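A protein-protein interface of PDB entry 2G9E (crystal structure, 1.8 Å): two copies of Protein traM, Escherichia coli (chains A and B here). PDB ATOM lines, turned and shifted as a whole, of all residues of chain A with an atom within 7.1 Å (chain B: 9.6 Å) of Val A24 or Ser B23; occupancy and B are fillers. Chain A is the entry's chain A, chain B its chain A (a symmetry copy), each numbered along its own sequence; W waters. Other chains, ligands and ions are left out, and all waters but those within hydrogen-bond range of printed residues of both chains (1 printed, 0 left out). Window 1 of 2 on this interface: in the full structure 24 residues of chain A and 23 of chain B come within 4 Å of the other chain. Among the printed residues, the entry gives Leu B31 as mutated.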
ATOM      1  N   VAL A  18      25.513   9.143  10.675  1.00  0.00           N
ATOM      2  CA  VAL A  18      24.691   8.104  11.302  1.00  0.00           C
ATOM      3  C   VAL A  18      25.015   7.978  12.792  1.00  0.00           C
ATOM      4  O   VAL A  18      24.103   7.883  13.634  1.00  0.00           O
ATOM      5  CB  VAL A  18      24.794   6.742  10.573  1.00  0.00           C
ATOM      6  CG1 VAL A  18      24.128   5.614  11.386  1.00  0.00           C
ATOM      7  CG2 VAL A  18      24.153   6.837   9.187  1.00  0.00           C
ATOM      8  N   LYS A  19      26.306   7.993  13.104  1.00  0.00           N
ATOM      9  CA  LYS A  19      26.767   7.939  14.474  1.00  0.00           C
ATOM     10  C   LYS A  19      26.299   9.180  15.252  1.00  0.00           C
ATOM     11  O   LYS A  19      25.865   9.072  16.388  1.00  0.00           O
ATOM     12  CB  LYS A  19      28.290   7.831  14.501  1.00  0.00           C
ATOM     13  CG  LYS A  19      28.870   7.442  15.849  1.00  0.00           C
ATOM     14  CD  LYS A  19      30.334   7.126  15.700  1.00  0.00           C
ATOM     15  CE  LYS A  19      30.831   6.347  16.881  1.00  0.00           C
ATOM     16  NZ  LYS A  19      32.309   6.129  16.751  1.00  0.00           N
ATOM     17  N   THR A  20      26.402  10.354  14.638  1.00  0.00           N
ATOM     18  CA  THR A  20      25.966  11.594  15.275  1.00  0.00           C
ATOM     19  C   THR A  20      24.465  11.534  15.599  1.00  0.00           C
ATOM     20  O   THR A  20      24.058  11.876  16.695  1.00  0.00           O
ATOM     21  CB  THR A  20      26.332  12.819  14.417  1.00  0.00           C
ATOM     22  OG1 THR A  20      27.750  13.037  14.471  1.00  0.00           O
ATOM     23  CG2 THR A  20      25.623  14.069  14.923  1.00  0.00           C
ATOM     24  N   GLN A  21      23.647  11.091  14.656  1.00  0.00           N
ATOM     25  CA  GLN A  21      22.200  11.072  14.846  1.00  0.00           C
ATOM     26  C   GLN A  21      21.818  10.119  15.983  1.00  0.00           C
ATOM     27  O   GLN A  21      20.972  10.448  16.826  1.00  0.00           O
ATOM     28  CB  GLN A  21      21.483  10.687  13.534  1.00  0.00           C
ATOM     29  CG  GLN A  21      19.972  10.435  13.645  1.00  0.00           C
ATOM     30  CD  GLN A  21      19.266  11.470  14.493  1.00  0.00           C
ATOM     31  OE1 GLN A  21      19.551  12.680  14.406  1.00  0.00           O
ATOM     32  NE2 GLN A  21      18.363  11.003  15.347  1.00  0.00           N
ATOM     33  N   SER A  22      22.430   8.934  15.976  1.00  0.00           N
ATOM     34  CA  SER A  22      22.189   7.929  17.011  1.00  0.00           C
ATOM     35  C   SER A  22      22.561   8.494  18.403  1.00  0.00           C
ATOM     36  O   SER A  22      21.850   8.273  19.390  1.00  0.00           O
ATOM     37  CB  SER A  22      22.958   6.646  16.695  1.00  0.00           C
ATOM     38  OG  SER A  22      22.624   5.600  17.617  1.00  0.00           O
ATOM     39  N   SER A  23      23.662   9.236  18.459  1.00  0.00           N
ATOM     40  CA  SER A  23      24.145   9.830  19.689  1.00  0.00           C
ATOM     41  C   SER A  23      23.252  10.978  20.157  1.00  0.00           C
ATOM     42  O   SER A  23      22.914  11.079  21.342  1.00  0.00           O
ATOM     43  CB  SER A  23      25.576  10.302  19.500  1.00  0.00           C
ATOM     44  OG  SER A  23      26.406   9.197  19.183  1.00  0.00           O
ATOM     45  N   VAL A  24      22.866  11.830  19.211  1.00  0.00           N
ATOM     46  CA  VAL A  24      21.994  12.979  19.475  1.00  0.00           C
ATOM     47  C   VAL A  24      20.594  12.562  19.957  1.00  0.00           C
ATOM     48  O   VAL A  24      19.983  13.209  20.810  1.00  0.00           O
ATOM     49  CB  VAL A  24      21.988  13.898  18.240  1.00  0.00           C
ATOM     50  CG1 VAL A  24      20.774  14.791  18.212  1.00  0.00           C
ATOM     51  CG2 VAL A  24      23.291  14.708  18.210  1.00  0.00           C
ATOM     52  N   ALA A  25      20.096  11.462  19.422  1.00  0.00           N
ATOM     53  CA  ALA A  25      18.833  10.897  19.905  1.00  0.00           C
ATOM     54  C   ALA A  25      18.913  10.529  21.414  1.00  0.00           C
ATOM     55  O   ALA A  25      17.943  10.699  22.167  1.00  0.00           O
ATOM     56  CB  ALA A  25      18.439   9.685  19.053  1.00  0.00           C
ATOM     57  N   LYS A  26      20.063  10.006  21.832  1.00  0.00           N
ATOM     58  CA  LYS A  26      20.279   9.656  23.238  1.00  0.00           C
ATOM     59  C   LYS A  26      20.460  10.904  24.097  1.00  0.00           C
ATOM     60  O   LYS A  26      19.899  10.996  25.191  1.00  0.00           O
ATOM     61  CB  LYS A  26      21.459   8.704  23.391  1.00  0.00           C
ATOM     62  CG  LYS A  26      21.189   7.368  22.770  1.00  0.00           C
ATOM     63  CD  LYS A  26      22.472   6.692  22.471  1.00  0.00           C
ATOM     64  CE  LYS A  26      22.255   5.221  22.332  1.00  0.00           C
ATOM     65  NZ  LYS A  26      20.971   4.903  21.670  1.00  0.00           N
ATOM     66  N   ILE A  27      21.238  11.856  23.587  1.00  0.00           N
ATOM     67  CA  ILE A  27      21.465  13.145  24.260  1.00  0.00           C
ATOM     68  C   ILE A  27      20.141  13.874  24.508  1.00  0.00           C
ATOM     69  O   ILE A  27      19.903  14.370  25.603  1.00  0.00           O
ATOM     70  CB  ILE A  27      22.436  14.030  23.454  1.00  0.00           C
ATOM     71  CG1 ILE A  27      23.849  13.413  23.478  1.00  0.00           C
ATOM     72  CG2 ILE A  27      22.444  15.489  24.002  1.00  0.00           C
ATOM     73  CD1 ILE A  27      24.742  13.831  22.297  1.00  0.00           C
ATOM     74  N   LEU A  28      19.295  13.953  23.484  1.00  0.00           N
ATOM     75  CA  LEU A  28      17.954  14.513  23.616  1.00  0.00           C
ATOM     76  C   LEU A  28      17.125  13.828  24.701  1.00  0.00           C
ATOM     77  O   LEU A  28      16.501  14.507  25.521  1.00  0.00           O
ATOM     78  CB  LEU A  28      17.222  14.451  22.266  1.00  0.00           C
ATOM     79  CG  LEU A  28      15.856  15.138  22.162  1.00  0.00           C
ATOM     80  CD1 LEU A  28      16.036  16.654  22.225  1.00  0.00           C
ATOM     81  CD2 LEU A  28      15.161  14.742  20.875  1.00  0.00           C
ATOM     82  N   GLY A  29      17.103  12.492  24.694  1.00  0.00           N
ATOM     83  CA  GLY A  29      16.437  11.702  25.726  1.00  0.00           C
ATOM     84  C   GLY A  29      16.903  12.007  27.140  1.00  0.00           C
ATOM     85  O   GLY A  29      16.073  12.209  28.048  1.00  0.00           O
ATOM     86  N   ILE A  30      18.223  12.054  27.329  1.00  0.00           N
ATOM     87  CA  ILE A  30      18.817  12.379  28.631  1.00  0.00           C
ATOM     88  C   ILE A  30      18.372  13.765  29.114  1.00  0.00           C
ATOM     89  O   ILE A  30      17.919  13.919  30.243  1.00  0.00           O
ATOM     90  CB  ILE A  30      20.368  12.301  28.603  1.00  0.00           C
ATOM     91  CG1 ILE A  30      20.842  10.855  28.375  1.00  0.00           C
ATOM     92  CG2 ILE A  30      20.963  12.847  29.917  1.00  0.00           C
ATOM     93  CD1 ILE A  30      22.369  10.694  28.169  1.00  0.00           C
ATOM     94  N   MET A  48       8.660  16.939  21.582  1.00  0.00           N
ATOM     95  CA  MET A  48       9.893  17.143  20.819  1.00  0.00           C
ATOM     96  C   MET A  48      10.020  16.137  19.695  1.00  0.00           C
ATOM     97  O   MET A  48      10.343  16.489  18.575  1.00  0.00           O
ATOM     98  CB  MET A  48      11.103  17.035  21.726  1.00  0.00           C
ATOM     99  CG  MET A  48      11.257  18.185  22.698  1.00  0.00           C
ATOM    100  SD  MET A  48      12.917  18.323  23.375  1.00  0.00           S
ATOM    101  CE  MET A  48      13.054  16.786  24.261  1.00  0.00           C
ATOM    102  N   ILE A  52      10.108  16.955  15.706  1.00  0.00           N
ATOM    103  CA  ILE A  52      11.256  16.500  14.930  1.00  0.00           C
ATOM    104  C   ILE A  52      10.743  15.695  13.731  1.00  0.00           C
ATOM    105  O   ILE A  52      11.206  15.878  12.600  1.00  0.00           O
ATOM    106  CB  ILE A  52      12.231  15.686  15.816  1.00  0.00           C
ATOM    107  CG1 ILE A  52      12.972  16.625  16.783  1.00  0.00           C
ATOM    108  CG2 ILE A  52      13.254  14.934  14.974  1.00  0.00           C
ATOM    109  CD1 ILE A  52      13.667  15.907  17.955  1.00  0.00           C
ATOM    110  N   GLU B  15      18.007  12.543   5.877  1.00  0.00           N
ATOM    111  CA  GLU B  15      17.263  12.242   7.089  1.00  0.00           C
ATOM    112  C   GLU B  15      18.122  12.471   8.344  1.00  0.00           C
ATOM    113  O   GLU B  15      17.673  13.103   9.283  1.00  0.00           O
ATOM    114  CB  GLU B  15      16.795  10.809   7.059  1.00  0.00           C
ATOM    115  CG  GLU B  15      16.087  10.387   8.321  1.00  0.00           C
ATOM    116  CD  GLU B  15      15.709   8.943   8.281  1.00  0.00           C
ATOM    117  OE1 GLU B  15      16.604   8.087   8.164  1.00  0.00           O
ATOM    118  OE2 GLU B  15      14.510   8.661   8.363  1.00  0.00           O
ATOM    119  N   CYS B  16      19.345  11.950   8.334  1.00  0.00           N
ATOM    120  CA  CYS B  16      20.244  12.063   9.479  1.00  0.00           C
ATOM    121  C   CYS B  16      20.526  13.532   9.789  1.00  0.00           C
ATOM    122  O   CYS B  16      20.378  13.966  10.956  1.00  0.00           O
ATOM    123  CB  CYS B  16      21.568  11.348   9.222  1.00  0.00           C
ATOM    124  SG  CYS B  16      21.465   9.566   9.277  1.00  0.00           S
ATOM    125  N   VAL B  17      20.937  14.290   8.769  1.00  0.00           N
ATOM    126  CA  VAL B  17      21.326  15.676   9.038  1.00  0.00           C
ATOM    127  C   VAL B  17      20.128  16.552   9.429  1.00  0.00           C
ATOM    128  O   VAL B  17      20.279  17.429  10.265  1.00  0.00           O
ATOM    129  CB  VAL B  17      22.224  16.322   7.927  1.00  0.00           C
ATOM    130  CG1 VAL B  17      23.455  15.452   7.652  1.00  0.00           C
ATOM    131  CG2 VAL B  17      21.448  16.643   6.638  1.00  0.00           C
ATOM    132  N   VAL B  18      18.947  16.305   8.851  1.00  0.00           N
ATOM    133  CA  VAL B  18      17.768  17.108   9.185  1.00  0.00           C
ATOM    134  C   VAL B  18      17.266  16.781  10.593  1.00  0.00           C
ATOM    135  O   VAL B  18      16.940  17.689  11.378  1.00  0.00           O
ATOM    136  CB  VAL B  18      16.643  16.983   8.129  1.00  0.00           C
ATOM    137  CG1 VAL B  18      15.332  17.629   8.619  1.00  0.00           C
ATOM    138  CG2 VAL B  18      17.083  17.627   6.812  1.00  0.00           C
ATOM    139  N   LYS B  19      17.221  15.490  10.902  1.00  0.00           N
ATOM    140  CA  LYS B  19      16.822  15.026  12.213  1.00  0.00           C
ATOM    141  C   LYS B  19      17.811  15.514  13.284  1.00  0.00           C
ATOM    142  O   LYS B  19      17.405  15.945  14.352  1.00  0.00           O
ATOM    143  CB  LYS B  19      16.737  13.501  12.216  1.00  0.00           C
ATOM    144  CG  LYS B  19      16.022  12.913  13.420  1.00  0.00           C
ATOM    145  CD  LYS B  19      15.780  11.444  13.198  1.00  0.00           C
ATOM    146  CE  LYS B  19      14.731  10.933  14.139  1.00  0.00           C
ATOM    147  NZ  LYS B  19      14.579   9.451  13.962  1.00  0.00           N
ATOM    148  N   THR B  20      19.105  15.433  12.995  1.00  0.00           N
ATOM    149  CA  THR B  20      20.131  15.889  13.930  1.00  0.00           C
ATOM    150  C   THR B  20      19.964  17.387  14.223  1.00  0.00           C
ATOM    151  O   THR B  20      20.003  17.799  15.369  1.00  0.00           O
ATOM    152  CB  THR B  20      21.543  15.545  13.420  1.00  0.00           C
ATOM    153  OG1 THR B  20      21.763  14.131  13.533  1.00  0.00           O
ATOM    154  CG2 THR B  20      22.607  16.275  14.229  1.00  0.00           C
ATOM    155  N   GLN B  21      19.766  18.199  13.194  1.00  0.00           N
ATOM    156  CA  GLN B  21      19.675  19.646  13.368  1.00  0.00           C
ATOM    157  C   GLN B  21      18.453  20.010  14.219  1.00  0.00           C
ATOM    158  O   GLN B  21      18.538  20.860  15.116  1.00  0.00           O
ATOM    159  CB  GLN B  21      19.630  20.358  11.999  1.00  0.00           C
ATOM    160  CG  GLN B  21      19.333  21.864  12.036  1.00  0.00           C
ATOM    161  CD  GLN B  21      20.100  22.586  13.121  1.00  0.00           C
ATOM    162  OE1 GLN B  21      21.296  22.323  13.351  1.00  0.00           O
ATOM    163  NE2 GLN B  21      19.413  23.480  13.822  1.00  0.00           N
ATOM    164  N   SER B  22      17.321  19.377  13.907  1.00  0.00           N
ATOM    165  CA  SER B  22      16.078  19.600  14.646  1.00  0.00           C
ATOM    166  C   SER B  22      16.270  19.236  16.138  1.00  0.00           C
ATOM    167  O   SER B  22      15.789  19.942  17.031  1.00  0.00           O
ATOM    168  CB  SER B  22      14.935  18.809  14.011  1.00  0.00           C
ATOM    169  OG  SER B  22      13.680  19.124  14.630  1.00  0.00           O
ATOM    170  N   SER B  23      16.990  18.148  16.388  1.00  0.00           N
ATOM    171  CA  SER B  23      17.254  17.674  17.731  1.00  0.00           C
ATOM    172  C   SER B  23      18.226  18.585  18.477  1.00  0.00           C
ATOM    173  O   SER B  23      18.011  18.923  19.647  1.00  0.00           O
ATOM    174  CB  SER B  23      17.783  16.251  17.676  1.00  0.00           C
ATOM    175  OG  SER B  23      16.812  15.403  17.086  1.00  0.00           O
ATOM    176  N   VAL B  24      19.288  18.987  17.783  1.00  0.00           N
ATOM    177  CA  VAL B  24      20.314  19.878  18.332  1.00  0.00           C
ATOM    178  C   VAL B  24      19.763  21.271  18.685  1.00  0.00           C
ATOM    179  O   VAL B  24      20.157  21.892  19.675  1.00  0.00           O
ATOM    180  CB  VAL B  24      21.521  19.902  17.378  1.00  0.00           C
ATOM    181  CG1 VAL B  24      22.370  21.131  17.578  1.00  0.00           C
ATOM    182  CG2 VAL B  24      22.334  18.613  17.563  1.00  0.00           C
ATOM    183  N   ALA B  25      18.830  21.751  17.882  1.00  0.00           N
ATOM    184  CA  ALA B  25      18.139  23.003  18.199  1.00  0.00           C
ATOM    185  C   ALA B  25      17.394  22.915  19.561  1.00  0.00           C
ATOM    186  O   ALA B  25      17.347  23.887  20.330  1.00  0.00           O
ATOM    187  CB  ALA B  25      17.182  23.377  17.061  1.00  0.00           C
ATOM    188  N   LYS B  26      16.800  21.755  19.833  1.00  0.00           N
ATOM    189  CA  LYS B  26      16.102  21.532  21.102  1.00  0.00           C
ATOM    190  C   LYS B  26      17.088  21.371  22.255  1.00  0.00           C
ATOM    191  O   LYS B  26      16.884  21.932  23.333  1.00  0.00           O
ATOM    192  CB  LYS B  26      15.162  20.336  21.007  1.00  0.00           C
ATOM    193  CG  LYS B  26      14.029  20.583  20.061  1.00  0.00           C
ATOM    194  CD  LYS B  26      13.475  19.289  19.600  1.00  0.00           C
ATOM    195  CE  LYS B  26      12.087  19.481  19.085  1.00  0.00           C
ATOM    196  NZ  LYS B  26      11.929  20.760  18.359  1.00  0.00           N
ATOM    197  N   ILE B  27      18.153  20.610  22.012  1.00  0.00           N
ATOM    198  CA  ILE B  27      19.227  20.405  22.995  1.00  0.00           C
ATOM    199  C   ILE B  27      19.845  21.741  23.420  1.00  0.00           C
ATOM    200  O   ILE B  27      20.036  21.986  24.605  1.00  0.00           O
ATOM    201  CB  ILE B  27      20.306  19.450  22.449  1.00  0.00           C
ATOM    202  CG1 ILE B  27      19.729  18.026  22.318  1.00  0.00           C
ATOM    203  CG2 ILE B  27      21.574  19.466  23.357  1.00  0.00           C
ATOM    204  CD1 ILE B  27      20.453  17.143  21.288  1.00  0.00           C
ATOM    205  N   LEU B  28      20.171  22.589  22.448  1.00  0.00           N
ATOM    206  CA  LEU B  28      20.656  23.939  22.716  1.00  0.00           C
ATOM    207  C   LEU B  28      19.699  24.756  23.584  1.00  0.00           C
ATOM    208  O   LEU B  28      20.131  25.389  24.550  1.00  0.00           O
ATOM    209  CB  LEU B  28      20.932  24.672  21.394  1.00  0.00           C
ATOM    210  CG  LEU B  28      21.600  26.050  21.467  1.00  0.00           C
ATOM    211  CD1 LEU B  28      23.050  25.896  21.920  1.00  0.00           C
ATOM    212  CD2 LEU B  28      21.539  26.739  20.119  1.00  0.00           C
ATOM    213  N   GLY B  29      18.410  24.754  23.232  1.00  0.00           N
ATOM    214  CA  GLY B  29      17.368  25.406  24.022  1.00  0.00           C
ATOM    215  C   GLY B  29      17.305  24.943  25.468  1.00  0.00           C
ATOM    216  O   GLY B  29      17.251  25.775  26.395  1.00  0.00           O
ATOM    217  N   ILE B  30      17.324  23.624  25.667  1.00  0.00           N
ATOM    218  CA  ILE B  30      17.311  23.034  27.011  1.00  0.00           C
ATOM    219  C   ILE B  30      18.517  23.502  27.834  1.00  0.00           C
ATOM    220  O   ILE B  30      18.365  23.956  28.963  1.00  0.00           O
ATOM    221  CB  ILE B  30      17.269  21.482  26.969  1.00  0.00           C
ATOM    222  CG1 ILE B  30      15.939  20.984  26.375  1.00  0.00           C
ATOM    223  CG2 ILE B  30      17.466  20.895  28.381  1.00  0.00           C
ATOM    224  CD1 ILE B  30      15.863  19.454  26.139  1.00  0.00           C
ATOM    225  N   LEU B  31      19.716  23.389  27.265  1.00  0.00           N
ATOM    226  CA  LEU B  31      20.953  23.734  27.971  1.00  0.00           C
ATOM    227  C   LEU B  31      21.118  25.225  28.254  1.00  0.00           C
ATOM    228  O   LEU B  31      21.762  25.613  29.231  1.00  0.00           O
ATOM    229  CB  LEU B  31      22.156  23.186  27.207  1.00  0.00           C
ATOM    230  CG  LEU B  31      22.299  21.668  27.319  1.00  0.00           C
ATOM    231  CD1 LEU B  31      23.420  21.211  26.405  1.00  0.00           C
ATOM    232  CD2 LEU B  31      22.550  21.225  28.768  1.00  0.00           C
HETATM  233  O   HOH W   1      17.121  12.745  17.447  1.00  0.00           O
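Thr B20 touches its own counterpart, Thr A20.
Val A24 touches Ile B27, but with the chains exchanged Ile A27 does not touch Val B24 (7.1 Å).
Ile A27 touches its own counterpart, Ile B27.
Leu A28 touches Ser B23, but with the chains exchanged Ser A23 does not touch Leu B28 (11.9 Å).
Positions printed for both chains: 18, 19, 20, 21, 22, 23, 24, 25, 26, 27, 28, 29 and 30.
Of the 16 pairs that touch across the chains among the printed residues, 2 have their exchanged pair printed and touching as well.
SG of Cys B16 touches CG2 of Val A18 (3.8 Å).
Thr B20 touches Thr A20 (CG2 to CG2, 3.8 Å).
Cys B16 touches Gln A21 (O to OE1, 3.8 Å).
CG1 of Val A24 touches CB of Ser B23, at 3.4 Å.
Val A24 touches Ile B27.
CD1 of Leu A28 touches O of Ser B23 (3.96 Å).
Met A48 touches Lys B26 (O to CE, 3.5 Å).
Lys B19 touches Ile A52.
OG of Ser B22 touches CG1 of Ile A52 (3.4 Å).
Ile A52 touches Ser B23.
Water W1 bridges the side-chain hydroxyl of Ser B23 (2.7 Å) and the side-chain amide nitrogen of Gln A21 (3.0 Å).
OG of Ser B23 is in hydrogen-bond range of O of Lys B19.
The backbone carbonyl oxygen of Cys B16 sits at hydrogen-bond distance from the side-chain hydroxyl of Thr B20 (2.9 Å).
The side-chain hydroxyl (OG1) of Thr B20 sits at hydrogen-bond distance from the side-chain amide oxygen (OE1) of Gln A21 (2.8 Å).
Of chain B, only Ser B23 (3.4 Å) and Ile B27 (3.9 Å) come within 4 Å of Val A24.
Of the printed residues of chain A, Ser B23 touches Val A24, Leu A28 and Ile A52.
Of the printed residues of chain B, Thr A20 touches Thr B20.
Of the printed residues of chain A, Lys B19 touches Gln A21 and Ile A52.
Of the printed residues of chain A, Cys B16 touches Val A18 and Gln A21.
Of the printed residues of chain A, Ile B27 touches Val A24, Ile A27 and Leu A28.
Printed residues of chain B within 4 Å of Met A48: Lys B26 (3.5 Å).
Val B18 touches none of the printed residues of chain A.
Lys A19 touches none of the printed residues of chain B.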
